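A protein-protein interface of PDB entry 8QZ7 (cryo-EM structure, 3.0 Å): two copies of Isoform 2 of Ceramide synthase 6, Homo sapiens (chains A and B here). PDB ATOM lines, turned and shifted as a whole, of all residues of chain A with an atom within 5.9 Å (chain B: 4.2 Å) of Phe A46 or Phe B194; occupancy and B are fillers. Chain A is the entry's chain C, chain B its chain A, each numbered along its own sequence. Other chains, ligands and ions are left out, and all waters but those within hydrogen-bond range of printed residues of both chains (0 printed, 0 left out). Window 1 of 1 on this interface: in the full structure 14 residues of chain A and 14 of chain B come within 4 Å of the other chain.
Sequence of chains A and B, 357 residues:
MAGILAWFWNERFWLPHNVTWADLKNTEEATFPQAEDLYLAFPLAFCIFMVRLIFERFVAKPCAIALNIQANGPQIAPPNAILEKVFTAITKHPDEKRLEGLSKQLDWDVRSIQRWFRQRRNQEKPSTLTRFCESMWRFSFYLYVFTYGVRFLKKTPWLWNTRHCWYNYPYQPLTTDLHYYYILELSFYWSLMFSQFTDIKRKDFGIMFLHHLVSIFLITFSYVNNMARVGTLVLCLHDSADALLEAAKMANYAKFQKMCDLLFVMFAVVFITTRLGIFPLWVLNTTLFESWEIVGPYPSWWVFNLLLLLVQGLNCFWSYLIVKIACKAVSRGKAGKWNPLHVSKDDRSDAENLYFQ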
ATOM      1  N   ALA A  41      41.179 -31.576  -5.867  1.00  0.00           N
ATOM      2  CA  ALA A  41      40.757 -30.183  -5.803  1.00  0.00           C
ATOM      3  C   ALA A  41      39.254 -30.020  -5.974  1.00  0.00           C
ATOM      4  O   ALA A  41      38.712 -28.982  -5.583  1.00  0.00           O
ATOM      5  CB  ALA A  41      41.486 -29.361  -6.865  1.00  0.00           C
ATOM      6  N   PHE A  42      38.570 -31.008  -6.551  1.00  0.00           N
ATOM      7  CA  PHE A  42      37.142 -30.864  -6.817  1.00  0.00           C
ATOM      8  C   PHE A  42      36.272 -31.140  -5.590  1.00  0.00           C
ATOM      9  O   PHE A  42      35.346 -30.363  -5.327  1.00  0.00           O
ATOM     10  CB  PHE A  42      36.725 -31.756  -7.986  1.00  0.00           C
ATOM     11  CG  PHE A  42      37.041 -31.171  -9.329  1.00  0.00           C
ATOM     12  CD1 PHE A  42      36.190 -30.249  -9.912  1.00  0.00           C
ATOM     13  CD2 PHE A  42      38.186 -31.540 -10.008  1.00  0.00           C
ATOM     14  CE1 PHE A  42      36.475 -29.710 -11.146  1.00  0.00           C
ATOM     15  CE2 PHE A  42      38.477 -31.003 -11.244  1.00  0.00           C
ATOM     16  CZ  PHE A  42      37.620 -30.087 -11.813  1.00  0.00           C
ATOM     17  N   PRO A  43      36.495 -32.219  -4.825  1.00  0.00           N
ATOM     18  CA  PRO A  43      35.719 -32.366  -3.582  1.00  0.00           C
ATOM     19  C   PRO A  43      35.987 -31.258  -2.581  1.00  0.00           C
ATOM     20  O   PRO A  43      35.039 -30.653  -2.066  1.00  0.00           O
ATOM     21  CB  PRO A  43      36.160 -33.736  -3.050  1.00  0.00           C
ATOM     22  CG  PRO A  43      37.449 -34.009  -3.707  1.00  0.00           C
ATOM     23  CD  PRO A  43      37.333 -33.406  -5.064  1.00  0.00           C
ATOM     24  N   LEU A  44      37.263 -30.960  -2.313  1.00  0.00           N
ATOM     25  CA  LEU A  44      37.601 -29.906  -1.364  1.00  0.00           C
ATOM     26  C   LEU A  44      36.952 -28.585  -1.741  1.00  0.00           C
ATOM     27  O   LEU A  44      36.420 -27.889  -0.866  1.00  0.00           O
ATOM     28  CB  LEU A  44      39.116 -29.742  -1.273  1.00  0.00           C
ATOM     29  CG  LEU A  44      39.891 -30.945  -0.741  1.00  0.00           C
ATOM     30  CD1 LEU A  44      41.379 -30.658  -0.740  1.00  0.00           C
ATOM     31  CD2 LEU A  44      39.416 -31.311   0.654  1.00  0.00           C
ATOM     32  N   ALA A  45      36.963 -28.237  -3.031  1.00  0.00           N
ATOM     33  CA  ALA A  45      36.279 -27.030  -3.478  1.00  0.00           C
ATOM     34  C   ALA A  45      34.837 -27.014  -2.999  1.00  0.00           C
ATOM     35  O   ALA A  45      34.392 -26.040  -2.379  1.00  0.00           O
ATOM     36  CB  ALA A  45      36.337 -26.926  -5.000  1.00  0.00           C
ATOM     37  N   PHE A  46      34.107 -28.110  -3.225  1.00  0.00           N
ATOM     38  CA  PHE A  46      32.736 -28.188  -2.737  1.00  0.00           C
ATOM     39  C   PHE A  46      32.690 -27.978  -1.233  1.00  0.00           C
ATOM     40  O   PHE A  46      31.888 -27.177  -0.735  1.00  0.00           O
ATOM     41  CB  PHE A  46      32.114 -29.531  -3.116  1.00  0.00           C
ATOM     42  CG  PHE A  46      30.699 -29.701  -2.641  1.00  0.00           C
ATOM     43  CD1 PHE A  46      29.661 -29.022  -3.256  1.00  0.00           C
ATOM     44  CD2 PHE A  46      30.405 -30.544  -1.581  1.00  0.00           C
ATOM     45  CE1 PHE A  46      28.359 -29.176  -2.822  1.00  0.00           C
ATOM     46  CE2 PHE A  46      29.105 -30.701  -1.144  1.00  0.00           C
ATOM     47  CZ  PHE A  46      28.082 -30.016  -1.765  1.00  0.00           C
ATOM     48  N   CYS A  47      33.589 -28.640  -0.498  1.00  0.00           N
ATOM     49  CA  CYS A  47      33.652 -28.429   0.943  1.00  0.00           C
ATOM     50  C   CYS A  47      33.862 -26.958   1.260  1.00  0.00           C
ATOM     51  O   CYS A  47      33.153 -26.390   2.101  1.00  0.00           O
ATOM     52  CB  CYS A  47      34.767 -29.276   1.555  1.00  0.00           C
ATOM     53  SG  CYS A  47      34.555 -31.056   1.357  1.00  0.00           S
ATOM     54  N   ILE A  48      34.792 -26.310   0.550  1.00  0.00           N
ATOM     55  CA  ILE A  48      35.009 -24.882   0.757  1.00  0.00           C
ATOM     56  C   ILE A  48      33.704 -24.130   0.565  1.00  0.00           C
ATOM     57  O   ILE A  48      33.302 -23.327   1.419  1.00  0.00           O
ATOM     58  CB  ILE A  48      36.108 -24.357  -0.185  1.00  0.00           C
ATOM     59  CG1 ILE A  48      37.476 -24.887   0.238  1.00  0.00           C
ATOM     60  CG2 ILE A  48      36.113 -22.839  -0.207  1.00  0.00           C
ATOM     61  CD1 ILE A  48      38.624 -24.294  -0.542  1.00  0.00           C
ATOM     62  N   PHE A  49      32.989 -24.433  -0.522  1.00  0.00           N
ATOM     63  CA  PHE A  49      31.708 -23.784  -0.760  1.00  0.00           C
ATOM     64  C   PHE A  49      30.787 -23.962   0.436  1.00  0.00           C
ATOM     65  O   PHE A  49      30.214 -22.984   0.935  1.00  0.00           O
ATOM     66  CB  PHE A  49      31.066 -24.337  -2.031  1.00  0.00           C
ATOM     67  CG  PHE A  49      29.779 -23.665  -2.398  1.00  0.00           C
ATOM     68  CD1 PHE A  49      29.782 -22.435  -3.029  1.00  0.00           C
ATOM     69  CD2 PHE A  49      28.565 -24.263  -2.113  1.00  0.00           C
ATOM     70  CE1 PHE A  49      28.599 -21.813  -3.367  1.00  0.00           C
ATOM     71  CE2 PHE A  49      27.379 -23.646  -2.449  1.00  0.00           C
ATOM     72  CZ  PHE A  49      27.397 -22.419  -3.077  1.00  0.00           C
ATOM     73  N   MET A  50      30.688 -25.193   0.954  1.00  0.00           N
ATOM     74  CA  MET A  50      29.867 -25.424   2.138  1.00  0.00           C
ATOM     75  C   MET A  50      30.281 -24.496   3.268  1.00  0.00           C
ATOM     76  O   MET A  50      29.444 -23.777   3.831  1.00  0.00           O
ATOM     77  CB  MET A  50      29.970 -26.883   2.582  1.00  0.00           C
ATOM     78  CG  MET A  50      29.347 -27.892   1.633  1.00  0.00           C
ATOM     79  SD  MET A  50      27.551 -27.783   1.553  1.00  0.00           S
ATOM     80  CE  MET A  50      27.322 -26.791   0.080  1.00  0.00           C
ATOM     81  N   VAL A  51      31.583 -24.450   3.567  1.00  0.00           N
ATOM     82  CA  VAL A  51      32.056 -23.594   4.646  1.00  0.00           C
ATOM     83  C   VAL A  51      31.662 -22.153   4.383  1.00  0.00           C
ATOM     84  O   VAL A  51      31.223 -21.445   5.299  1.00  0.00           O
ATOM     85  CB  VAL A  51      33.578 -23.743   4.826  1.00  0.00           C
ATOM     86  CG1 VAL A  51      34.051 -22.899   5.993  1.00  0.00           C
ATOM     87  CG2 VAL A  51      33.943 -25.199   5.036  1.00  0.00           C
ATOM     88  N   SER A 191      35.896 -23.223  -6.319  1.00  0.00           N
ATOM     89  CA  SER A 191      34.791 -22.731  -5.505  1.00  0.00           C
ATOM     90  C   SER A 191      34.190 -21.466  -6.100  1.00  0.00           C
ATOM     91  O   SER A 191      32.964 -21.299  -6.122  1.00  0.00           O
ATOM     92  CB  SER A 191      35.269 -22.472  -4.078  1.00  0.00           C
ATOM     93  OG  SER A 191      34.452 -21.511  -3.440  1.00  0.00           O
ATOM     94  N   PHE A 194      32.106 -22.491  -9.043  1.00  0.00           N
ATOM     95  CA  PHE A 194      30.825 -23.029  -8.595  1.00  0.00           C
ATOM     96  C   PHE A 194      29.873 -21.909  -8.198  1.00  0.00           C
ATOM     97  O   PHE A 194      28.709 -21.893  -8.609  1.00  0.00           O
ATOM     98  CB  PHE A 194      31.029 -23.991  -7.422  1.00  0.00           C
ATOM     99  CG  PHE A 194      31.771 -25.249  -7.781  1.00  0.00           C
ATOM    100  CD1 PHE A 194      31.933 -25.630  -9.101  1.00  0.00           C
ATOM    101  CD2 PHE A 194      32.299 -26.057  -6.789  1.00  0.00           C
ATOM    102  CE1 PHE A 194      32.615 -26.786  -9.425  1.00  0.00           C
ATOM    103  CE2 PHE A 194      32.979 -27.214  -7.107  1.00  0.00           C
ATOM    104  CZ  PHE A 194      33.138 -27.579  -8.427  1.00  0.00           C
ATOM    105  N   THR A 198      26.367 -22.012 -10.805  1.00  0.00           N
ATOM    106  CA  THR A 198      25.115 -22.584 -10.337  1.00  0.00           C
ATOM    107  C   THR A 198      24.430 -21.789  -9.239  1.00  0.00           C
ATOM    108  O   THR A 198      23.202 -21.819  -9.162  1.00  0.00           O
ATOM    109  CB  THR A 198      25.339 -24.020  -9.838  1.00  0.00           C
ATOM    110  OG1 THR A 198      24.239 -24.423  -9.013  1.00  0.00           O
ATOM    111  CG2 THR A 198      26.626 -24.127  -9.050  1.00  0.00           C
ATOM    112  N   ALA B  45      30.664 -35.059 -12.345  1.00  0.00           N
ATOM    113  CA  ALA B  45      29.393 -34.545 -11.851  1.00  0.00           C
ATOM    114  C   ALA B  45      29.182 -33.105 -12.289  1.00  0.00           C
ATOM    115  O   ALA B  45      28.143 -32.773 -12.875  1.00  0.00           O
ATOM    116  CB  ALA B  45      29.335 -34.654 -10.330  1.00  0.00           C
ATOM    117  N   PHE B  46      30.182 -32.248 -12.066  1.00  0.00           N
ATOM    118  CA  PHE B  46      30.073 -30.866 -12.518  1.00  0.00           C
ATOM    119  C   PHE B  46      29.820 -30.810 -14.015  1.00  0.00           C
ATOM    120  O   PHE B  46      28.913 -30.103 -14.472  1.00  0.00           O
ATOM    121  CB  PHE B  46      31.337 -30.088 -12.150  1.00  0.00           C
ATOM    122  CG  PHE B  46      31.314 -28.651 -12.590  1.00  0.00           C
ATOM    123  CD1 PHE B  46      30.524 -27.724 -11.931  1.00  0.00           C
ATOM    124  CD2 PHE B  46      32.085 -28.226 -13.658  1.00  0.00           C
ATOM    125  CE1 PHE B  46      30.502 -26.403 -12.330  1.00  0.00           C
ATOM    126  CE2 PHE B  46      32.065 -26.906 -14.062  1.00  0.00           C
ATOM    127  CZ  PHE B  46      31.272 -25.994 -13.398  1.00  0.00           C
ATOM    128  N   TRP B 190      25.894 -36.923  -7.222  1.00  0.00           N
ATOM    129  CA  TRP B 190      26.567 -35.679  -6.863  1.00  0.00           C
ATOM    130  C   TRP B 190      26.033 -34.498  -7.662  1.00  0.00           C
ATOM    131  O   TRP B 190      25.969 -33.379  -7.144  1.00  0.00           O
ATOM    132  CB  TRP B 190      28.076 -35.814  -7.048  1.00  0.00           C
ATOM    133  CG  TRP B 190      28.743 -36.560  -5.940  1.00  0.00           C
ATOM    134  CD1 TRP B 190      29.479 -37.698  -6.050  1.00  0.00           C
ATOM    135  CD2 TRP B 190      28.727 -36.226  -4.548  1.00  0.00           C
ATOM    136  NE1 TRP B 190      29.930 -38.091  -4.815  1.00  0.00           N
ATOM    137  CE2 TRP B 190      29.481 -37.204  -3.875  1.00  0.00           C
ATOM    138  CE3 TRP B 190      28.152 -35.190  -3.805  1.00  0.00           C
ATOM    139  CZ2 TRP B 190      29.673 -37.180  -2.498  1.00  0.00           C
ATOM    140  CZ3 TRP B 190      28.344 -35.168  -2.438  1.00  0.00           C
ATOM    141  CH2 TRP B 190      29.098 -36.156  -1.799  1.00  0.00           C
ATOM    142  N   SER B 191      25.642 -34.722  -8.918  1.00  0.00           N
ATOM    143  CA  SER B 191      24.993 -33.668  -9.689  1.00  0.00           C
ATOM    144  C   SER B 191      23.677 -33.247  -9.049  1.00  0.00           C
ATOM    145  O   SER B 191      23.358 -32.054  -8.990  1.00  0.00           O
ATOM    146  CB  SER B 191      24.761 -34.139 -11.122  1.00  0.00           C
ATOM    147  OG  SER B 191      23.686 -33.435 -11.716  1.00  0.00           O
ATOM    148  N   LEU B 192      22.895 -34.217  -8.574  1.00  0.00           N
ATOM    149  CA  LEU B 192      21.659 -33.885  -7.870  1.00  0.00           C
ATOM    150  C   LEU B 192      21.945 -33.097  -6.598  1.00  0.00           C
ATOM    151  O   LEU B 192      21.233 -32.138  -6.279  1.00  0.00           O
ATOM    152  CB  LEU B 192      20.874 -35.152  -7.541  1.00  0.00           C
ATOM    153  CG  LEU B 192      20.268 -35.899  -8.725  1.00  0.00           C
ATOM    154  CD1 LEU B 192      19.307 -36.961  -8.228  1.00  0.00           C
ATOM    155  CD2 LEU B 192      19.572 -34.931  -9.663  1.00  0.00           C
ATOM    156  N   MET B 193      22.983 -33.491  -5.858  1.00  0.00           N
ATOM    157  CA  MET B 193      23.347 -32.751  -4.654  1.00  0.00           C
ATOM    158  C   MET B 193      23.763 -31.321  -4.978  1.00  0.00           C
ATOM    159  O   MET B 193      23.418 -30.392  -4.238  1.00  0.00           O
ATOM    160  CB  MET B 193      24.470 -33.475  -3.911  1.00  0.00           C
ATOM    161  CG  MET B 193      24.318 -33.503  -2.397  1.00  0.00           C
ATOM    162  SD  MET B 193      23.368 -34.907  -1.778  1.00  0.00           S
ATOM    163  CE  MET B 193      21.689 -34.324  -1.977  1.00  0.00           C
ATOM    164  N   PHE B 194      24.505 -31.125  -6.071  1.00  0.00           N
ATOM    165  CA  PHE B 194      24.864 -29.775  -6.495  1.00  0.00           C
ATOM    166  C   PHE B 194      23.623 -28.964  -6.840  1.00  0.00           C
ATOM    167  O   PHE B 194      23.471 -27.822  -6.397  1.00  0.00           O
ATOM    168  CB  PHE B 194      25.815 -29.826  -7.694  1.00  0.00           C
ATOM    169  CG  PHE B 194      27.165 -30.410  -7.385  1.00  0.00           C
ATOM    170  CD1 PHE B 194      27.596 -30.556  -6.078  1.00  0.00           C
ATOM    171  CD2 PHE B 194      28.008 -30.806  -8.409  1.00  0.00           C
ATOM    172  CE1 PHE B 194      28.838 -31.094  -5.800  1.00  0.00           C
ATOM    173  CE2 PHE B 194      29.250 -31.342  -8.135  1.00  0.00           C
ATOM    174  CZ  PHE B 194      29.665 -31.487  -6.829  1.00  0.00           C
ATOM    175  N   SER B 195      22.714 -29.546  -7.626  1.00  0.00           N
ATOM    176  CA  SER B 195      21.496 -28.833  -7.997  1.00  0.00           C
ATOM    177  C   SER B 195      20.617 -28.527  -6.793  1.00  0.00           C
ATOM    178  O   SER B 195      19.845 -27.563  -6.832  1.00  0.00           O
ATOM    179  CB  SER B 195      20.703 -29.636  -9.027  1.00  0.00           C
ATOM    180  OG  SER B 195      21.446 -29.817 -10.219  1.00  0.00           O
ATOM    181  N   GLN B 196      20.707 -29.325  -5.732  1.00  0.00           N
ATOM    182  CA  GLN B 196      19.934 -29.090  -4.518  1.00  0.00           C
ATOM    183  C   GLN B 196      20.553 -28.043  -3.605  1.00  0.00           C
ATOM    184  O   GLN B 196      19.826 -27.237  -3.017  1.00  0.00           O
ATOM    185  CB  GLN B 196      19.766 -30.401  -3.740  1.00  0.00           C
ATOM    186  CG  GLN B 196      19.043 -30.263  -2.407  1.00  0.00           C
ATOM    187  CD  GLN B 196      17.540 -30.133  -2.561  1.00  0.00           C
ATOM    188  OE1 GLN B 196      17.019 -30.046  -3.672  1.00  0.00           O
ATOM    189  NE2 GLN B 196      16.833 -30.127  -1.439  1.00  0.00           N
ATOM    190  N   PHE B 197      21.879 -28.025  -3.475  1.00  0.00           N
ATOM    191  CA  PHE B 197      22.507 -27.141  -2.498  1.00  0.00           C
ATOM    192  C   PHE B 197      22.646 -25.717  -3.022  1.00  0.00           C
ATOM    193  O   PHE B 197      22.119 -24.773  -2.423  1.00  0.00           O
ATOM    194  CB  PHE B 197      23.877 -27.686  -2.092  1.00  0.00           C
ATOM    195  CG  PHE B 197      23.878 -28.398  -0.774  1.00  0.00           C
ATOM    196  CD1 PHE B 197      24.026 -29.772  -0.712  1.00  0.00           C
ATOM    197  CD2 PHE B 197      23.723 -27.691   0.403  1.00  0.00           C
ATOM    198  CE1 PHE B 197      24.026 -30.427   0.502  1.00  0.00           C
ATOM    199  CE2 PHE B 197      23.721 -28.340   1.620  1.00  0.00           C
ATOM    200  CZ  PHE B 197      23.873 -29.710   1.669  1.00  0.00           C
ATOM    201  N   THR B 198      23.347 -25.541  -4.138  1.00  0.00           N
ATOM    202  CA  THR B 198      23.745 -24.214  -4.583  1.00  0.00           C
ATOM    203  C   THR B 198      22.843 -23.609  -5.645  1.00  0.00           C
ATOM    204  O   THR B 198      22.713 -22.385  -5.688  1.00  0.00           O
ATOM    205  CB  THR B 198      25.184 -24.241  -5.120  1.00  0.00           C
ATOM    206  OG1 THR B 198      25.423 -23.079  -5.922  1.00  0.00           O
ATOM    207  CG2 THR B 198      25.433 -25.485  -5.947  1.00  0.00           C
ATOM    208  N   ASP B 199      22.204 -24.422  -6.488  1.00  0.00           N
ATOM    209  CA  ASP B 199      21.432 -23.866  -7.596  1.00  0.00           C
ATOM    210  C   ASP B 199      20.296 -22.986  -7.088  1.00  0.00           C
ATOM    211  O   ASP B 199      20.107 -21.860  -7.560  1.00  0.00           O
ATOM    212  CB  ASP B 199      20.898 -24.987  -8.485  1.00  0.00           C
ATOM    213  CG  ASP B 199      20.247 -24.463  -9.749  1.00  0.00           C
ATOM    214  OD1 ASP B 199      20.976 -23.957 -10.628  1.00  0.00           O
ATOM    215  OD2 ASP B 199      19.006 -24.551  -9.861  1.00  0.00           O
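OG1 of Thr A198 sits close to N of Asp B199, 3.2 Å away.
Among the printed residues, merely in contact across the chains: Phe A46 with Phe B194, Phe A49 with Thr B198, Met A50 with Phe B197, Phe A194 with Phe B46 and Thr A198 with Thr B198.
Phe A46 touches just one residue of chain B: Phe B194 (3.4 Å). Of the printed residues of chain B, Phe A49 touches Thr B198. Of the printed residues of chain A, Phe B46 touches Phe A194 (3.4 Å). Met B193 touches none of the printed residues of chain A. Phe B194 touches one residue of chain A. The nearest printed residue of chain A that does not touch Phe B197 is Phe A46 (4.2 Å).
Of the 12 printed residues of chain B, 5 touch a printed residue of chain A. Hydrophobic or aromatic side chains of chain B that line the printed part of chain A: Phe B46, Phe B194 and Phe B197. Printed residues of chain A that touch a printed residue of chain B: Phe A46, Phe A49, Met A50, Phe A194 and Thr A198. Hydrophobic or aromatic side chains of chain A within 4 Å of the printed part of chain B: Phe A46, Phe A49, Met A50 and Phe A194.
Phe A46 touches Phe B194, and with the chains exchanged Phe A194 touches Phe B46. Thr B198 touches its own counterpart, Thr A198. 5 positions are printed for both chains. Of the 6 pairs that touch across the chains among the printed residues, 3 have their exchanged pair printed and touching as well.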
